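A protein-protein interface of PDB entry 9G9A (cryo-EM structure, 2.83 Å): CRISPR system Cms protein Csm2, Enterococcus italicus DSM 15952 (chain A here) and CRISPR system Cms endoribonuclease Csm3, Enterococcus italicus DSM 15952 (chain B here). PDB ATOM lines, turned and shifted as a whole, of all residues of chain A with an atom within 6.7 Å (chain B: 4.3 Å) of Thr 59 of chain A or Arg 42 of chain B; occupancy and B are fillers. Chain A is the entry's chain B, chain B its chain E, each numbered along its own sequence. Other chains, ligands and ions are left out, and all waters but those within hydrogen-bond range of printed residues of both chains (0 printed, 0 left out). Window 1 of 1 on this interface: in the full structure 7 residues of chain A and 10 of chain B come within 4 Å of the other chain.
The backbone carbonyl oxygen (O) of Tyr 40 of chain B is in hydrogen-bond range of the side-chain hydroxyl (OH) of Tyr 62 of chain A (3.0 Å).
The backbone carbonyl oxygen of Asn 55 of chain A is in hydrogen-bond range of the side-chain hydroxyl of Thr 59 of chain A, 3.0 Å away.
The backbone carbonyl oxygen (O) of His 56 of chain A sits at hydrogen-bond distance from the side-chain hydroxyl (OG1) of Thr 59 of chain A, 2.6 Å away.
The backbone carbonyl oxygen (O) of Thr 59 of chain A lies close to the side-chain amide oxygen (OD1) of Asn 63 of chain A (2.9 Å).
The guanidinium group (NH1) of Arg 37 of chain B sits at hydrogen-bond distance from the backbone carbonyl oxygen (O) of Arg 42 of chain B, at 2.6 Å.
The side-chain hydroxyl (OG) of Ser 41 of chain B lies within hydrogen-bond range of the side-chain carboxylate (OD2) of Asp 38 of chain B (2.9 Å).
Among the printed residues, merely in contact across the chains: Tyr 58 of chain A with Arg 42 of chain B, Tyr 62 of chain A with Arg 42 of chain B, Tyr 62 of chain A with Pro 39 of chain B, Tyr 62 of chain A with Ser 41 of chain B and Thr 59 of chain A with Arg 42 of chain B.
Of chain B, only Arg 42 comes within 4 Å of Thr 59 of chain A.
Of the printed residues of chain A, Arg 42 of chain B touches Tyr 58 (3.5 Å), Thr 59 (3.9 Å) and Tyr 62 (3.5 Å).
Of the printed residues of chain A, Ser 41 of chain B touches Tyr 62 (3.8 Å).
Of the printed residues of chain A, Tyr 40 of chain B touches Tyr 62.
Of the printed residues of chain B, Tyr 62 of chain A touches Pro 39 (3.7 Å), Tyr 40 (3.0 Å), Ser 41 (3.8 Å) and Arg 42 (3.5 Å).
Of the printed residues of chain A, Pro 39 of chain B touches Tyr 62 (3.7 Å).
Val 57 of chain A touches none of the printed residues of chain B.
Val 61 of chain A touches none of the printed residues of chain B.
The nearest printed residue of chain B that does not touch Thr 59 of chain A is Arg 37 of chain B (5.5 Å).
Printed residues of chain A that touch a printed residue of chain B: Tyr 58, Thr 59 and Tyr 62.
Hydrophobic or aromatic side chains of chain A within 4 Å of the printed part of chain B: Tyr 58 and Tyr 62.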
ATOM      1  N   ILE A  54      19.156   8.750  10.601  1.00  0.00           N
ATOM      2  CA  ILE A  54      20.078   8.042  11.482  1.00  0.00           C
ATOM      3  C   ILE A  54      20.520   8.943  12.629  1.00  0.00           C
ATOM      4  O   ILE A  54      20.670   8.487  13.767  1.00  0.00           O
ATOM      5  CB  ILE A  54      21.275   7.499  10.680  1.00  0.00           C
ATOM      6  CG1 ILE A  54      20.809   6.415   9.705  1.00  0.00           C
ATOM      7  CG2 ILE A  54      22.339   6.941  11.608  1.00  0.00           C
ATOM      8  CD1 ILE A  54      21.926   5.797   8.898  1.00  0.00           C
ATOM      9  N   ASN A  55      20.721  10.235  12.357  1.00  0.00           N
ATOM     10  CA  ASN A  55      21.058  11.179  13.417  1.00  0.00           C
ATOM     11  C   ASN A  55      19.923  11.325  14.419  1.00  0.00           C
ATOM     12  O   ASN A  55      20.172  11.414  15.625  1.00  0.00           O
ATOM     13  CB  ASN A  55      21.411  12.545  12.823  1.00  0.00           C
ATOM     14  CG  ASN A  55      22.762  12.553  12.137  1.00  0.00           C
ATOM     15  OD1 ASN A  55      22.903  13.057  11.023  1.00  0.00           O
ATOM     16  ND2 ASN A  55      23.767  11.998  12.803  1.00  0.00           N
ATOM     17  N   HIS A  56      18.677  11.365  13.942  1.00  0.00           N
ATOM     18  CA  HIS A  56      17.541  11.443  14.855  1.00  0.00           C
ATOM     19  C   HIS A  56      17.495  10.224  15.770  1.00  0.00           C
ATOM     20  O   HIS A  56      17.340  10.351  16.993  1.00  0.00           O
ATOM     21  CB  HIS A  56      16.241  11.577  14.060  1.00  0.00           C
ATOM     22  CG  HIS A  56      15.043  11.891  14.903  1.00  0.00           C
ATOM     23  ND1 HIS A  56      15.138  12.224  16.236  1.00  0.00           N
ATOM     24  CD2 HIS A  56      13.725  11.925  14.599  1.00  0.00           C
ATOM     25  CE1 HIS A  56      13.928  12.449  16.718  1.00  0.00           C
ATOM     26  NE2 HIS A  56      13.053  12.274  15.745  1.00  0.00           N
ATOM     27  N   VAL A  57      17.655   9.029  15.194  1.00  0.00           N
ATOM     28  CA  VAL A  57      17.625   7.814  16.007  1.00  0.00           C
ATOM     29  C   VAL A  57      18.800   7.790  16.979  1.00  0.00           C
ATOM     30  O   VAL A  57      18.658   7.380  18.139  1.00  0.00           O
ATOM     31  CB  VAL A  57      17.604   6.561  15.112  1.00  0.00           C
ATOM     32  CG1 VAL A  57      17.404   5.315  15.957  1.00  0.00           C
ATOM     33  CG2 VAL A  57      16.501   6.667  14.076  1.00  0.00           C
ATOM     34  N   TYR A  58      19.978   8.224  16.523  1.00  0.00           N
ATOM     35  CA  TYR A  58      21.155   8.249  17.384  1.00  0.00           C
ATOM     36  C   TYR A  58      20.965   9.200  18.557  1.00  0.00           C
ATOM     37  O   TYR A  58      21.334   8.877  19.691  1.00  0.00           O
ATOM     38  CB  TYR A  58      22.385   8.645  16.564  1.00  0.00           C
ATOM     39  CG  TYR A  58      23.658   8.784  17.368  1.00  0.00           C
ATOM     40  CD1 TYR A  58      24.065  10.020  17.854  1.00  0.00           C
ATOM     41  CD2 TYR A  58      24.457   7.682  17.635  1.00  0.00           C
ATOM     42  CE1 TYR A  58      25.228  10.152  18.588  1.00  0.00           C
ATOM     43  CE2 TYR A  58      25.621   7.805  18.366  1.00  0.00           C
ATOM     44  CZ  TYR A  58      26.003   9.041  18.840  1.00  0.00           C
ATOM     45  OH  TYR A  58      27.161   9.166  19.569  1.00  0.00           O
ATOM     46  N   THR A  59      20.401  10.383  18.302  1.00  0.00           N
ATOM     47  CA  THR A  59      20.138  11.325  19.384  1.00  0.00           C
ATOM     48  C   THR A  59      19.120  10.761  20.365  1.00  0.00           C
ATOM     49  O   THR A  59      19.272  10.911  21.584  1.00  0.00           O
ATOM     50  CB  THR A  59      19.655  12.660  18.820  1.00  0.00           C
ATOM     51  OG1 THR A  59      18.577  12.433  17.903  1.00  0.00           O
ATOM     52  CG2 THR A  59      20.787  13.381  18.102  1.00  0.00           C
ATOM     53  N   LYS A  60      18.076  10.104  19.853  1.00  0.00           N
ATOM     54  CA  LYS A  60      17.083   9.506  20.740  1.00  0.00           C
ATOM     55  C   LYS A  60      17.704   8.424  21.617  1.00  0.00           C
ATOM     56  O   LYS A  60      17.387   8.324  22.809  1.00  0.00           O
ATOM     57  CB  LYS A  60      15.921   8.940  19.926  1.00  0.00           C
ATOM     58  CG  LYS A  60      15.101  10.001  19.214  1.00  0.00           C
ATOM     59  CD  LYS A  60      13.986   9.381  18.397  1.00  0.00           C
ATOM     60  CE  LYS A  60      13.025   8.612  19.281  1.00  0.00           C
ATOM     61  NZ  LYS A  60      11.903   8.040  18.494  1.00  0.00           N
ATOM     62  N   VAL A  61      18.584   7.601  21.045  1.00  0.00           N
ATOM     63  CA  VAL A  61      19.251   6.566  21.832  1.00  0.00           C
ATOM     64  C   VAL A  61      20.183   7.188  22.866  1.00  0.00           C
ATOM     65  O   VAL A  61      20.204   6.775  24.031  1.00  0.00           O
ATOM     66  CB  VAL A  61      20.000   5.591  20.906  1.00  0.00           C
ATOM     67  CG1 VAL A  61      20.863   4.642  21.720  1.00  0.00           C
ATOM     68  CG2 VAL A  61      19.018   4.809  20.059  1.00  0.00           C
ATOM     69  N   TYR A  62      20.964   8.193  22.459  1.00  0.00           N
ATOM     70  CA  TYR A  62      21.930   8.811  23.361  1.00  0.00           C
ATOM     71  C   TYR A  62      21.237   9.499  24.530  1.00  0.00           C
ATOM     72  O   TYR A  62      21.739   9.468  25.661  1.00  0.00           O
ATOM     73  CB  TYR A  62      22.797   9.804  22.586  1.00  0.00           C
ATOM     74  CG  TYR A  62      23.937  10.403  23.381  1.00  0.00           C
ATOM     75  CD1 TYR A  62      25.193   9.813  23.385  1.00  0.00           C
ATOM     76  CD2 TYR A  62      23.760  11.567  24.117  1.00  0.00           C
ATOM     77  CE1 TYR A  62      26.238  10.361  24.105  1.00  0.00           C
ATOM     78  CE2 TYR A  62      24.797  12.118  24.842  1.00  0.00           C
ATOM     79  CZ  TYR A  62      26.034  11.515  24.831  1.00  0.00           C
ATOM     80  OH  TYR A  62      27.067  12.068  25.550  1.00  0.00           O
ATOM     81  N   ASN A  63      20.089  10.134  24.277  1.00  0.00           N
ATOM     82  CA  ASN A  63      19.360  10.795  25.356  1.00  0.00           C
ATOM     83  C   ASN A  63      18.928   9.797  26.423  1.00  0.00           C
ATOM     84  O   ASN A  63      19.005  10.087  27.622  1.00  0.00           O
ATOM     85  CB  ASN A  63      18.149  11.539  24.792  1.00  0.00           C
ATOM     86  CG  ASN A  63      18.542  12.743  23.959  1.00  0.00           C
ATOM     87  OD1 ASN A  63      19.708  12.910  23.599  1.00  0.00           O
ATOM     88  ND2 ASN A  63      17.569  13.589  23.645  1.00  0.00           N
ATOM     89  N   SER A  64      18.473   8.619  26.008  1.00  0.00           N
ATOM     90  CA  SER A  64      18.077   7.578  26.949  1.00  0.00           C
ATOM     91  C   SER A  64      19.299   6.884  27.542  1.00  0.00           C
ATOM     92  O   SER A  64      20.375   6.884  26.946  1.00  0.00           O
ATOM     93  CB  SER A  64      17.170   6.553  26.266  1.00  0.00           C
ATOM     94  OG  SER A  64      15.981   7.161  25.793  1.00  0.00           O
ATOM     95  N   PHE A 119      23.902  -0.665  18.274  1.00  0.00           N
ATOM     96  CA  PHE A 119      23.456   0.476  17.482  1.00  0.00           C
ATOM     97  C   PHE A 119      24.524   1.559  17.406  1.00  0.00           C
ATOM     98  O   PHE A 119      24.675   2.208  16.365  1.00  0.00           O
ATOM     99  CB  PHE A 119      22.161   1.054  18.048  1.00  0.00           C
ATOM    100  CG  PHE A 119      21.660   2.250  17.292  1.00  0.00           C
ATOM    101  CD1 PHE A 119      21.240   2.125  15.979  1.00  0.00           C
ATOM    102  CD2 PHE A 119      21.620   3.498  17.888  1.00  0.00           C
ATOM    103  CE1 PHE A 119      20.785   3.221  15.275  1.00  0.00           C
ATOM    104  CE2 PHE A 119      21.163   4.597  17.190  1.00  0.00           C
ATOM    105  CZ  PHE A 119      20.747   4.457  15.882  1.00  0.00           C
ATOM    106  N   ARG B  37      26.953  22.848  21.054  1.00  0.00           N
ATOM    107  CA  ARG B  37      26.166  21.891  21.815  1.00  0.00           C
ATOM    108  C   ARG B  37      26.878  21.554  23.114  1.00  0.00           C
ATOM    109  O   ARG B  37      28.109  21.584  23.191  1.00  0.00           O
ATOM    110  CB  ARG B  37      25.918  20.605  21.016  1.00  0.00           C
ATOM    111  CG  ARG B  37      25.005  20.774  19.819  1.00  0.00           C
ATOM    112  CD  ARG B  37      24.913  19.486  19.020  1.00  0.00           C
ATOM    113  NE  ARG B  37      23.886  19.551  17.988  1.00  0.00           N
ATOM    114  CZ  ARG B  37      22.645  19.109  18.139  1.00  0.00           C
ATOM    115  NH1 ARG B  37      22.239  18.562  19.272  1.00  0.00           N
ATOM    116  NH2 ARG B  37      21.790  19.217  17.128  1.00  0.00           N
ATOM    117  N   ASP B  38      26.093  21.238  24.133  1.00  0.00           N
ATOM    118  CA  ASP B  38      26.652  20.780  25.396  1.00  0.00           C
ATOM    119  C   ASP B  38      27.208  19.377  25.205  1.00  0.00           C
ATOM    120  O   ASP B  38      26.451  18.469  24.840  1.00  0.00           O
ATOM    121  CB  ASP B  38      25.582  20.799  26.483  1.00  0.00           C
ATOM    122  CG  ASP B  38      26.073  20.228  27.797  1.00  0.00           C
ATOM    123  OD1 ASP B  38      27.062  20.755  28.345  1.00  0.00           O
ATOM    124  OD2 ASP B  38      25.465  19.255  28.289  1.00  0.00           O
ATOM    125  N   PRO B  39      28.508  19.151  25.423  1.00  0.00           N
ATOM    126  CA  PRO B  39      29.076  17.826  25.117  1.00  0.00           C
ATOM    127  C   PRO B  39      28.449  16.687  25.902  1.00  0.00           C
ATOM    128  O   PRO B  39      28.296  15.584  25.363  1.00  0.00           O
ATOM    129  CB  PRO B  39      30.562  18.004  25.463  1.00  0.00           C
ATOM    130  CG  PRO B  39      30.803  19.470  25.357  1.00  0.00           C
ATOM    131  CD  PRO B  39      29.541  20.115  25.832  1.00  0.00           C
ATOM    132  N   TYR B  40      28.078  16.922  27.162  1.00  0.00           N
ATOM    133  CA  TYR B  40      27.597  15.830  28.003  1.00  0.00           C
ATOM    134  C   TYR B  40      26.270  15.275  27.499  1.00  0.00           C
ATOM    135  O   TYR B  40      26.054  14.058  27.515  1.00  0.00           O
ATOM    136  CB  TYR B  40      27.468  16.300  29.451  1.00  0.00           C
ATOM    137  CG  TYR B  40      27.164  15.182  30.420  1.00  0.00           C
ATOM    138  CD1 TYR B  40      28.116  14.217  30.714  1.00  0.00           C
ATOM    139  CD2 TYR B  40      25.927  15.090  31.041  1.00  0.00           C
ATOM    140  CE1 TYR B  40      27.846  13.192  31.598  1.00  0.00           C
ATOM    141  CE2 TYR B  40      25.648  14.069  31.927  1.00  0.00           C
ATOM    142  CZ  TYR B  40      26.610  13.123  32.202  1.00  0.00           C
ATOM    143  OH  TYR B  40      26.336  12.104  33.085  1.00  0.00           O
ATOM    144  N   SER B  41      25.371  16.148  27.049  1.00  0.00           N
ATOM    145  CA  SER B  41      24.051  15.739  26.591  1.00  0.00           C
ATOM    146  C   SER B  41      23.876  15.844  25.081  1.00  0.00           C
ATOM    147  O   SER B  41      22.855  15.384  24.561  1.00  0.00           O
ATOM    148  CB  SER B  41      22.970  16.569  27.292  1.00  0.00           C
ATOM    149  OG  SER B  41      23.172  17.953  27.079  1.00  0.00           O
ATOM    150  N   ARG B  42      24.841  16.432  24.370  1.00  0.00           N
ATOM    151  CA  ARG B  42      24.770  16.612  22.916  1.00  0.00           C
ATOM    152  C   ARG B  42      23.542  17.419  22.508  1.00  0.00           C
ATOM    153  O   ARG B  42      23.046  17.299  21.386  1.00  0.00           O
ATOM    154  CB  ARG B  42      24.806  15.267  22.183  1.00  0.00           C
ATOM    155  CG  ARG B  42      26.024  14.421  22.515  1.00  0.00           C
ATOM    156  CD  ARG B  42      26.069  13.138  21.697  1.00  0.00           C
ATOM    157  NE  ARG B  42      26.591  13.353  20.354  1.00  0.00           N
ATOM    158  CZ  ARG B  42      25.841  13.510  19.272  1.00  0.00           C
ATOM    159  NH1 ARG B  42      24.521  13.479  19.335  1.00  0.00           N
ATOM    160  NH2 ARG B  42      26.433  13.699  18.095  1.00  0.00           N
ATOM    161  N   LEU B  43      23.040  18.251  23.427  1.00  0.00           N
ATOM    162  CA  LEU B  43      21.935  19.174  23.236  1.00  0.00           C
ATOM    163  C   LEU B  43      22.457  20.574  22.943  1.00  0.00           C
ATOM    164  O   LEU B  43      23.521  20.962  23.436  1.00  0.00           O
ATOM    165  CB  LEU B  43      21.042  19.219  24.480  1.00  0.00           C
ATOM    166  CG  LEU B  43      19.749  18.401  24.471  1.00  0.00           C
ATOM    167  CD1 LEU B  43      20.024  16.930  24.234  1.00  0.00           C
ATOM    168  CD2 LEU B  43      19.015  18.600  25.779  1.00  0.00           C
